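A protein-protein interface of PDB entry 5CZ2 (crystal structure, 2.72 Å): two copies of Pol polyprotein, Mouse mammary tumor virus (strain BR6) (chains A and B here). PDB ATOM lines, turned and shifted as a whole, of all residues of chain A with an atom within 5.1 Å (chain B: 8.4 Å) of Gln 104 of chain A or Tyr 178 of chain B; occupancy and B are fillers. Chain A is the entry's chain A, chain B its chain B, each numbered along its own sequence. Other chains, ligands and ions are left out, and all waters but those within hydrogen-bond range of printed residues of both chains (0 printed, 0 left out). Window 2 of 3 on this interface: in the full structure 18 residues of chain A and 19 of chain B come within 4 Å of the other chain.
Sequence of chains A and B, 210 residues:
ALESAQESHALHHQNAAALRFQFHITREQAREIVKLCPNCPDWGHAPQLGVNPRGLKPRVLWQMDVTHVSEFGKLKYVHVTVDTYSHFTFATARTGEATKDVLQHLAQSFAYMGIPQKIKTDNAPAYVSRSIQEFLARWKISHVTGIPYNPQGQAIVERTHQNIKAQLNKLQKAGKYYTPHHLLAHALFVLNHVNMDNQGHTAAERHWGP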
ATOM      1  N   ARG A  94      23.873 -20.389  -9.697  1.00  0.00           N
ATOM      2  CA  ARG A  94      22.987 -19.784  -8.713  1.00  0.00           C
ATOM      3  C   ARG A  94      22.534 -20.829  -7.703  1.00  0.00           C
ATOM      4  O   ARG A  94      22.732 -22.033  -7.883  1.00  0.00           O
ATOM      5  CB  ARG A  94      21.776 -19.129  -9.387  1.00  0.00           C
ATOM      6  CG  ARG A  94      22.150 -18.103 -10.441  1.00  0.00           C
ATOM      7  CD  ARG A  94      20.960 -17.270 -10.870  1.00  0.00           C
ATOM      8  NE  ARG A  94      21.350 -16.235 -11.824  1.00  0.00           N
ATOM      9  CZ  ARG A  94      21.888 -15.070 -11.480  1.00  0.00           C
ATOM     10  NH1 ARG A  94      22.104 -14.787 -10.202  1.00  0.00           N
ATOM     11  NH2 ARG A  94      22.213 -14.186 -12.414  1.00  0.00           N
ATOM     12  N   LYS A 100      13.105 -15.966  -9.111  1.00  0.00           N
ATOM     13  CA  LYS A 100      14.070 -14.925  -8.774  1.00  0.00           C
ATOM     14  C   LYS A 100      15.408 -15.171  -9.461  1.00  0.00           C
ATOM     15  O   LYS A 100      16.069 -14.227  -9.908  1.00  0.00           O
ATOM     16  CB  LYS A 100      14.244 -14.852  -7.256  1.00  0.00           C
ATOM     17  CG  LYS A 100      15.487 -14.108  -6.794  1.00  0.00           C
ATOM     18  CD  LYS A 100      15.481 -13.906  -5.285  1.00  0.00           C
ATOM     19  CE  LYS A 100      15.258 -15.217  -4.543  1.00  0.00           C
ATOM     20  NZ  LYS A 100      16.341 -16.206  -4.801  1.00  0.00           N
ATOM     21  N   ASP A 101      15.818 -16.436  -9.563  1.00  0.00           N
ATOM     22  CA  ASP A 101      17.094 -16.755 -10.194  1.00  0.00           C
ATOM     23  C   ASP A 101      17.043 -16.522 -11.699  1.00  0.00           C
ATOM     24  O   ASP A 101      17.994 -15.986 -12.282  1.00  0.00           O
ATOM     25  CB  ASP A 101      17.479 -18.200  -9.886  1.00  0.00           C
ATOM     26  CG  ASP A 101      17.523 -18.485  -8.397  1.00  0.00           C
ATOM     27  OD1 ASP A 101      18.079 -17.657  -7.648  1.00  0.00           O
ATOM     28  OD2 ASP A 101      16.990 -19.534  -7.976  1.00  0.00           O
ATOM     29  N   VAL A 102      15.947 -16.923 -12.346  1.00  0.00           N
ATOM     30  CA  VAL A 102      15.841 -16.792 -13.796  1.00  0.00           C
ATOM     31  C   VAL A 102      15.830 -15.323 -14.206  1.00  0.00           C
ATOM     32  O   VAL A 102      16.467 -14.937 -15.194  1.00  0.00           O
ATOM     33  CB  VAL A 102      14.594 -17.537 -14.307  1.00  0.00           C
ATOM     34  CG1 VAL A 102      14.383 -17.274 -15.790  1.00  0.00           C
ATOM     35  CG2 VAL A 102      14.721 -19.029 -14.036  1.00  0.00           C
ATOM     36  N   LEU A 103      15.112 -14.482 -13.456  1.00  0.00           N
ATOM     37  CA  LEU A 103      15.035 -13.064 -13.796  1.00  0.00           C
ATOM     38  C   LEU A 103      16.408 -12.405 -13.756  1.00  0.00           C
ATOM     39  O   LEU A 103      16.742 -11.597 -14.631  1.00  0.00           O
ATOM     40  CB  LEU A 103      14.069 -12.348 -12.850  1.00  0.00           C
ATOM     41  CG  LEU A 103      12.580 -12.545 -13.135  1.00  0.00           C
ATOM     42  CD1 LEU A 103      11.732 -11.950 -12.027  1.00  0.00           C
ATOM     43  CD2 LEU A 103      12.224 -11.916 -14.469  1.00  0.00           C
ATOM     44  N   GLN A 104      17.217 -12.732 -12.748  1.00  0.00           N
ATOM     45  CA  GLN A 104      18.548 -12.143 -12.660  1.00  0.00           C
ATOM     46  C   GLN A 104      19.464 -12.680 -13.753  1.00  0.00           C
ATOM     47  O   GLN A 104      20.244 -11.923 -14.344  1.00  0.00           O
ATOM     48  CB  GLN A 104      19.145 -12.398 -11.277  1.00  0.00           C
ATOM     49  CG  GLN A 104      18.299 -11.853 -10.136  1.00  0.00           C
ATOM     50  CD  GLN A 104      19.009 -11.923  -8.800  1.00  0.00           C
ATOM     51  OE1 GLN A 104      20.225 -11.749  -8.720  1.00  0.00           O
ATOM     52  NE2 GLN A 104      18.251 -12.181  -7.740  1.00  0.00           N
ATOM     53  N   HIS A 105      19.391 -13.985 -14.032  1.00  0.00           N
ATOM     54  CA  HIS A 105      20.168 -14.548 -15.131  1.00  0.00           C
ATOM     55  C   HIS A 105      19.778 -13.932 -16.467  1.00  0.00           C
ATOM     56  O   HIS A 105      20.632 -13.761 -17.345  1.00  0.00           O
ATOM     57  CB  HIS A 105      19.997 -16.066 -15.181  1.00  0.00           C
ATOM     58  CG  HIS A 105      20.706 -16.710 -16.332  1.00  0.00           C
ATOM     59  ND1 HIS A 105      22.063 -16.953 -16.329  1.00  0.00           N
ATOM     60  CD2 HIS A 105      20.248 -17.155 -17.525  1.00  0.00           C
ATOM     61  CE1 HIS A 105      22.409 -17.524 -17.468  1.00  0.00           C
ATOM     62  NE2 HIS A 105      21.326 -17.659 -18.212  1.00  0.00           N
ATOM     63  N   LEU A 106      18.496 -13.602 -16.646  1.00  0.00           N
ATOM     64  CA  LEU A 106      18.063 -12.969 -17.886  1.00  0.00           C
ATOM     65  C   LEU A 106      18.677 -11.583 -18.037  1.00  0.00           C
ATOM     66  O   LEU A 106      19.130 -11.213 -19.126  1.00  0.00           O
ATOM     67  CB  LEU A 106      16.538 -12.888 -17.930  1.00  0.00           C
ATOM     68  CG  LEU A 106      15.793 -14.162 -18.328  1.00  0.00           C
ATOM     69  CD1 LEU A 106      14.299 -13.999 -18.104  1.00  0.00           C
ATOM     70  CD2 LEU A 106      16.086 -14.520 -19.777  1.00  0.00           C
ATOM     71  N   ALA A 107      18.690 -10.801 -16.955  1.00  0.00           N
ATOM     72  CA  ALA A 107      19.336  -9.493 -16.993  1.00  0.00           C
ATOM     73  C   ALA A 107      20.823  -9.623 -17.301  1.00  0.00           C
ATOM     74  O   ALA A 107      21.371  -8.843 -18.088  1.00  0.00           O
ATOM     75  CB  ALA A 107      19.121  -8.764 -15.667  1.00  0.00           C
ATOM     76  N   GLN A 108      21.492 -10.598 -16.683  1.00  0.00           N
ATOM     77  CA  GLN A 108      22.914 -10.802 -16.940  1.00  0.00           C
ATOM     78  C   GLN A 108      23.161 -11.239 -18.379  1.00  0.00           C
ATOM     79  O   GLN A 108      24.143 -10.817 -19.002  1.00  0.00           O
ATOM     80  CB  GLN A 108      23.481 -11.828 -15.962  1.00  0.00           C
ATOM     81  CG  GLN A 108      23.469 -11.382 -14.510  1.00  0.00           C
ATOM     82  CD  GLN A 108      24.852 -11.393 -13.890  1.00  0.00           C
ATOM     83  OE1 GLN A 108      25.239 -12.352 -13.222  1.00  0.00           O
ATOM     84  NE2 GLN A 108      25.607 -10.321 -14.109  1.00  0.00           N
ATOM     85  N   SER A 109      22.289 -12.097 -18.918  1.00  0.00           N
ATOM     86  CA  SER A 109      22.396 -12.494 -20.319  1.00  0.00           C
ATOM     87  C   SER A 109      22.329 -11.287 -21.246  1.00  0.00           C
ATOM     88  O   SER A 109      23.059 -11.218 -22.243  1.00  0.00           O
ATOM     89  CB  SER A 109      21.298 -13.497 -20.667  1.00  0.00           C
ATOM     90  OG  SER A 109      21.405 -14.670 -19.880  1.00  0.00           O
ATOM     91  N   LYS B 176      11.507  -1.321  -9.914  1.00  0.00           N
ATOM     92  CA  LYS B 176      12.231  -1.935  -8.808  1.00  0.00           C
ATOM     93  C   LYS B 176      13.044  -3.136  -9.284  1.00  0.00           C
ATOM     94  O   LYS B 176      12.625  -3.863 -10.185  1.00  0.00           O
ATOM     95  CB  LYS B 176      11.263  -2.358  -7.701  1.00  0.00           C
ATOM     96  N   TYR B 177      14.209  -3.333  -8.676  1.00  0.00           N
ATOM     97  CA  TYR B 177      15.097  -4.445  -8.984  1.00  0.00           C
ATOM     98  C   TYR B 177      15.225  -5.361  -7.772  1.00  0.00           C
ATOM     99  O   TYR B 177      14.772  -5.042  -6.669  1.00  0.00           O
ATOM    100  CB  TYR B 177      16.474  -3.937  -9.426  1.00  0.00           C
ATOM    101  CG  TYR B 177      16.439  -3.161 -10.724  1.00  0.00           C
ATOM    102  CD1 TYR B 177      16.589  -3.804 -11.944  1.00  0.00           C
ATOM    103  CD2 TYR B 177      16.239  -1.786 -10.728  1.00  0.00           C
ATOM    104  CE1 TYR B 177      16.552  -3.100 -13.133  1.00  0.00           C
ATOM    105  CE2 TYR B 177      16.201  -1.072 -11.911  1.00  0.00           C
ATOM    106  CZ  TYR B 177      16.358  -1.735 -13.110  1.00  0.00           C
ATOM    107  OH  TYR B 177      16.319  -1.029 -14.291  1.00  0.00           O
ATOM    108  N   TYR B 178      15.853  -6.516  -7.990  1.00  0.00           N
ATOM    109  CA  TYR B 178      15.997  -7.520  -6.939  1.00  0.00           C
ATOM    110  C   TYR B 178      17.238  -7.271  -6.086  1.00  0.00           C
ATOM    111  O   TYR B 178      17.144  -7.142  -4.862  1.00  0.00           O
ATOM    112  CB  TYR B 178      16.048  -8.924  -7.553  1.00  0.00           C
ATOM    113  CG  TYR B 178      14.690  -9.536  -7.803  1.00  0.00           C
ATOM    114  CD1 TYR B 178      14.109  -9.501  -9.062  1.00  0.00           C
ATOM    115  CD2 TYR B 178      13.989 -10.150  -6.774  1.00  0.00           C
ATOM    116  CE1 TYR B 178      12.866 -10.060  -9.291  1.00  0.00           C
ATOM    117  CE2 TYR B 178      12.746 -10.713  -6.992  1.00  0.00           C
ATOM    118  CZ  TYR B 178      12.190 -10.665  -8.252  1.00  0.00           C
ATOM    119  OH  TYR B 178      10.952 -11.224  -8.473  1.00  0.00           O
ATOM    120  N   THR B 179      18.401  -7.205  -6.719  1.00  0.00           N
ATOM    121  CA  THR B 179      19.682  -6.992  -6.062  1.00  0.00           C
ATOM    122  C   THR B 179      20.469  -5.950  -6.834  1.00  0.00           C
ATOM    123  O   THR B 179      20.124  -5.610  -7.971  1.00  0.00           O
ATOM    124  CB  THR B 179      20.480  -8.305  -5.986  1.00  0.00           C
ATOM    125  OG1 THR B 179      20.581  -8.882  -7.294  1.00  0.00           O
ATOM    126  CG2 THR B 179      19.807  -9.294  -5.046  1.00  0.00           C
ATOM    127  N   PRO B 180      21.535  -5.405  -6.238  1.00  0.00           N
ATOM    128  CA  PRO B 180      22.445  -4.549  -7.017  1.00  0.00           C
ATOM    129  C   PRO B 180      22.985  -5.220  -8.268  1.00  0.00           C
ATOM    130  O   PRO B 180      23.299  -4.528  -9.246  1.00  0.00           O
ATOM    131  CB  PRO B 180      23.570  -4.226  -6.020  1.00  0.00           C
ATOM    132  CG  PRO B 180      23.313  -5.083  -4.807  1.00  0.00           C
ATOM    133  CD  PRO B 180      21.856  -5.376  -4.803  1.00  0.00           C
ATOM    134  N   HIS B 181      23.117  -6.549  -8.264  1.00  0.00           N
ATOM    135  CA  HIS B 181      23.502  -7.264  -9.476  1.00  0.00           C
ATOM    136  C   HIS B 181      22.473  -7.054 -10.581  1.00  0.00           C
ATOM    137  O   HIS B 181      22.827  -6.802 -11.739  1.00  0.00           O
ATOM    138  CB  HIS B 181      23.669  -8.754  -9.174  1.00  0.00           C
ATOM    139  CG  HIS B 181      24.609  -9.042  -8.045  1.00  0.00           C
ATOM    140  ND1 HIS B 181      25.873  -8.498  -7.972  1.00  0.00           N
ATOM    141  CD2 HIS B 181      24.467  -9.814  -6.942  1.00  0.00           C
ATOM    142  CE1 HIS B 181      26.471  -8.925  -6.874  1.00  0.00           C
ATOM    143  NE2 HIS B 181      25.639  -9.724  -6.230  1.00  0.00           N
ATOM    144  N   HIS B 182      21.187  -7.170 -10.238  1.00  0.00           N
ATOM    145  CA  HIS B 182      20.117  -6.938 -11.206  1.00  0.00           C
ATOM    146  C   HIS B 182      20.194  -5.532 -11.788  1.00  0.00           C
ATOM    147  O   HIS B 182      20.159  -5.350 -13.011  1.00  0.00           O
ATOM    148  CB  HIS B 182      18.760  -7.177 -10.542  1.00  0.00           C
ATOM    149  CG  HIS B 182      17.640  -7.411 -11.509  1.00  0.00           C
ATOM    150  ND1 HIS B 182      17.682  -6.982 -12.818  1.00  0.00           N
ATOM    151  CD2 HIS B 182      16.443  -8.026 -11.353  1.00  0.00           C
ATOM    152  CE1 HIS B 182      16.561  -7.325 -13.428  1.00  0.00           C
ATOM    153  NE2 HIS B 182      15.792  -7.960 -12.561  1.00  0.00           N
ATOM    154  N   LEU B 183      20.278  -4.521 -10.920  1.00  0.00           N
ATOM    155  CA  LEU B 183      20.356  -3.137 -11.381  1.00  0.00           C
ATOM    156  C   LEU B 183      21.566  -2.925 -12.285  1.00  0.00           C
ATOM    157  O   LEU B 183      21.461  -2.296 -13.344  1.00  0.00           O
ATOM    158  CB  LEU B 183      20.409  -2.193 -10.178  1.00  0.00           C
ATOM    159  CG  LEU B 183      19.585  -0.903 -10.225  1.00  0.00           C
ATOM    160  CD1 LEU B 183      19.829  -0.079  -8.971  1.00  0.00           C
ATOM    161  CD2 LEU B 183      19.881  -0.087 -11.472  1.00  0.00           C
ATOM    162  N   ALA B 185      23.405  -5.094 -14.075  1.00  0.00           N
ATOM    163  CA  ALA B 185      23.246  -5.761 -15.364  1.00  0.00           C
ATOM    164  C   ALA B 185      22.433  -4.912 -16.333  1.00  0.00           C
ATOM    165  O   ALA B 185      22.791  -4.781 -17.510  1.00  0.00           O
ATOM    166  CB  ALA B 185      22.594  -7.130 -15.173  1.00  0.00           C
ATOM    167  N   HIS B 186      21.329  -4.334 -15.857  1.00  0.00           N
ATOM    168  CA  HIS B 186      20.505  -3.483 -16.710  1.00  0.00           C
ATOM    169  C   HIS B 186      21.278  -2.247 -17.151  1.00  0.00           C
ATOM    170  O   HIS B 186      21.256  -1.873 -18.329  1.00  0.00           O
ATOM    171  CB  HIS B 186      19.224  -3.091 -15.969  1.00  0.00           C
ATOM    172  CG  HIS B 186      18.174  -2.481 -16.847  1.00  0.00           C
ATOM    173  ND1 HIS B 186      16.864  -2.333 -16.442  1.00  0.00           N
ATOM    174  CD2 HIS B 186      18.235  -1.988 -18.106  1.00  0.00           C
ATOM    175  CE1 HIS B 186      16.166  -1.771 -17.412  1.00  0.00           C
ATOM    176  NE2 HIS B 186      16.974  -1.551 -18.433  1.00  0.00           N
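The side-chain amide oxygen (OE1) of Gln 104 of chain A is in hydrogen-bond range of the side-chain hydroxyl (OG1) of Thr 179 of chain B (3.2 Å).
Along chain B the printed residues that touch a printed residue of chain A span positions 178 to 185.
Of the 11 printed residues of chain A, 4 touch a printed residue of chain B.
Among the printed residues, no Asp or Glu carboxylate lies within 4 Å of a Lys or Arg side-chain nitrogen of the other chain.
Of the printed residues of chain B, Leu 103 of chain A touches Tyr 178.
Of the printed residues of chain B, Gln 104 of chain A touches Tyr 178 and Thr 179.
Tyr 178 of chain B touches just these residues of chain A: Leu 103 and Gln 104.
Of the printed residues of chain A, Thr 179 of chain B touches Gln 104 (3.2 Å).
Pro 180 of chain B touches none of the printed residues of chain A.
Printed residues of chain A within 4 Å of His 182 of chain B: Ala 107.
Printed residues of chain A within 4 Å of Ala 185 of chain B: Ala 107 (3.6 Å) and Gln 108 (3.9 Å).
The nearest residue of chain B that does not touch Gln 104 of chain A is His 182 of chain B (4.4 Å).
The nearest residue of chain A that does not touch Tyr 178 of chain B is Lys 100 of chain A (4.2 Å).
Among the printed residues, merely in contact across the chains: Leu 103 of chain A with Tyr 178 of chain B (3.5 Å), Ala 107 of chain A with Ala 185 of chain B (3.6 Å), Ala 107 of chain A with His 182 of chain B (3.7 Å), Gln 104 of chain A with Tyr 178 of chain B (3.9 Å) and Gln 108 of chain A with Ala 185 of chain B (3.9 Å).
No position is printed for both chains.
Of the 6 pairs that touch across the chains among the printed residues, none has its exchanged pair printed and touching as well.
OG1 of Thr 179 of chain B sits at hydrogen-bond distance from N of His 182 of chain B (3.5 Å).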
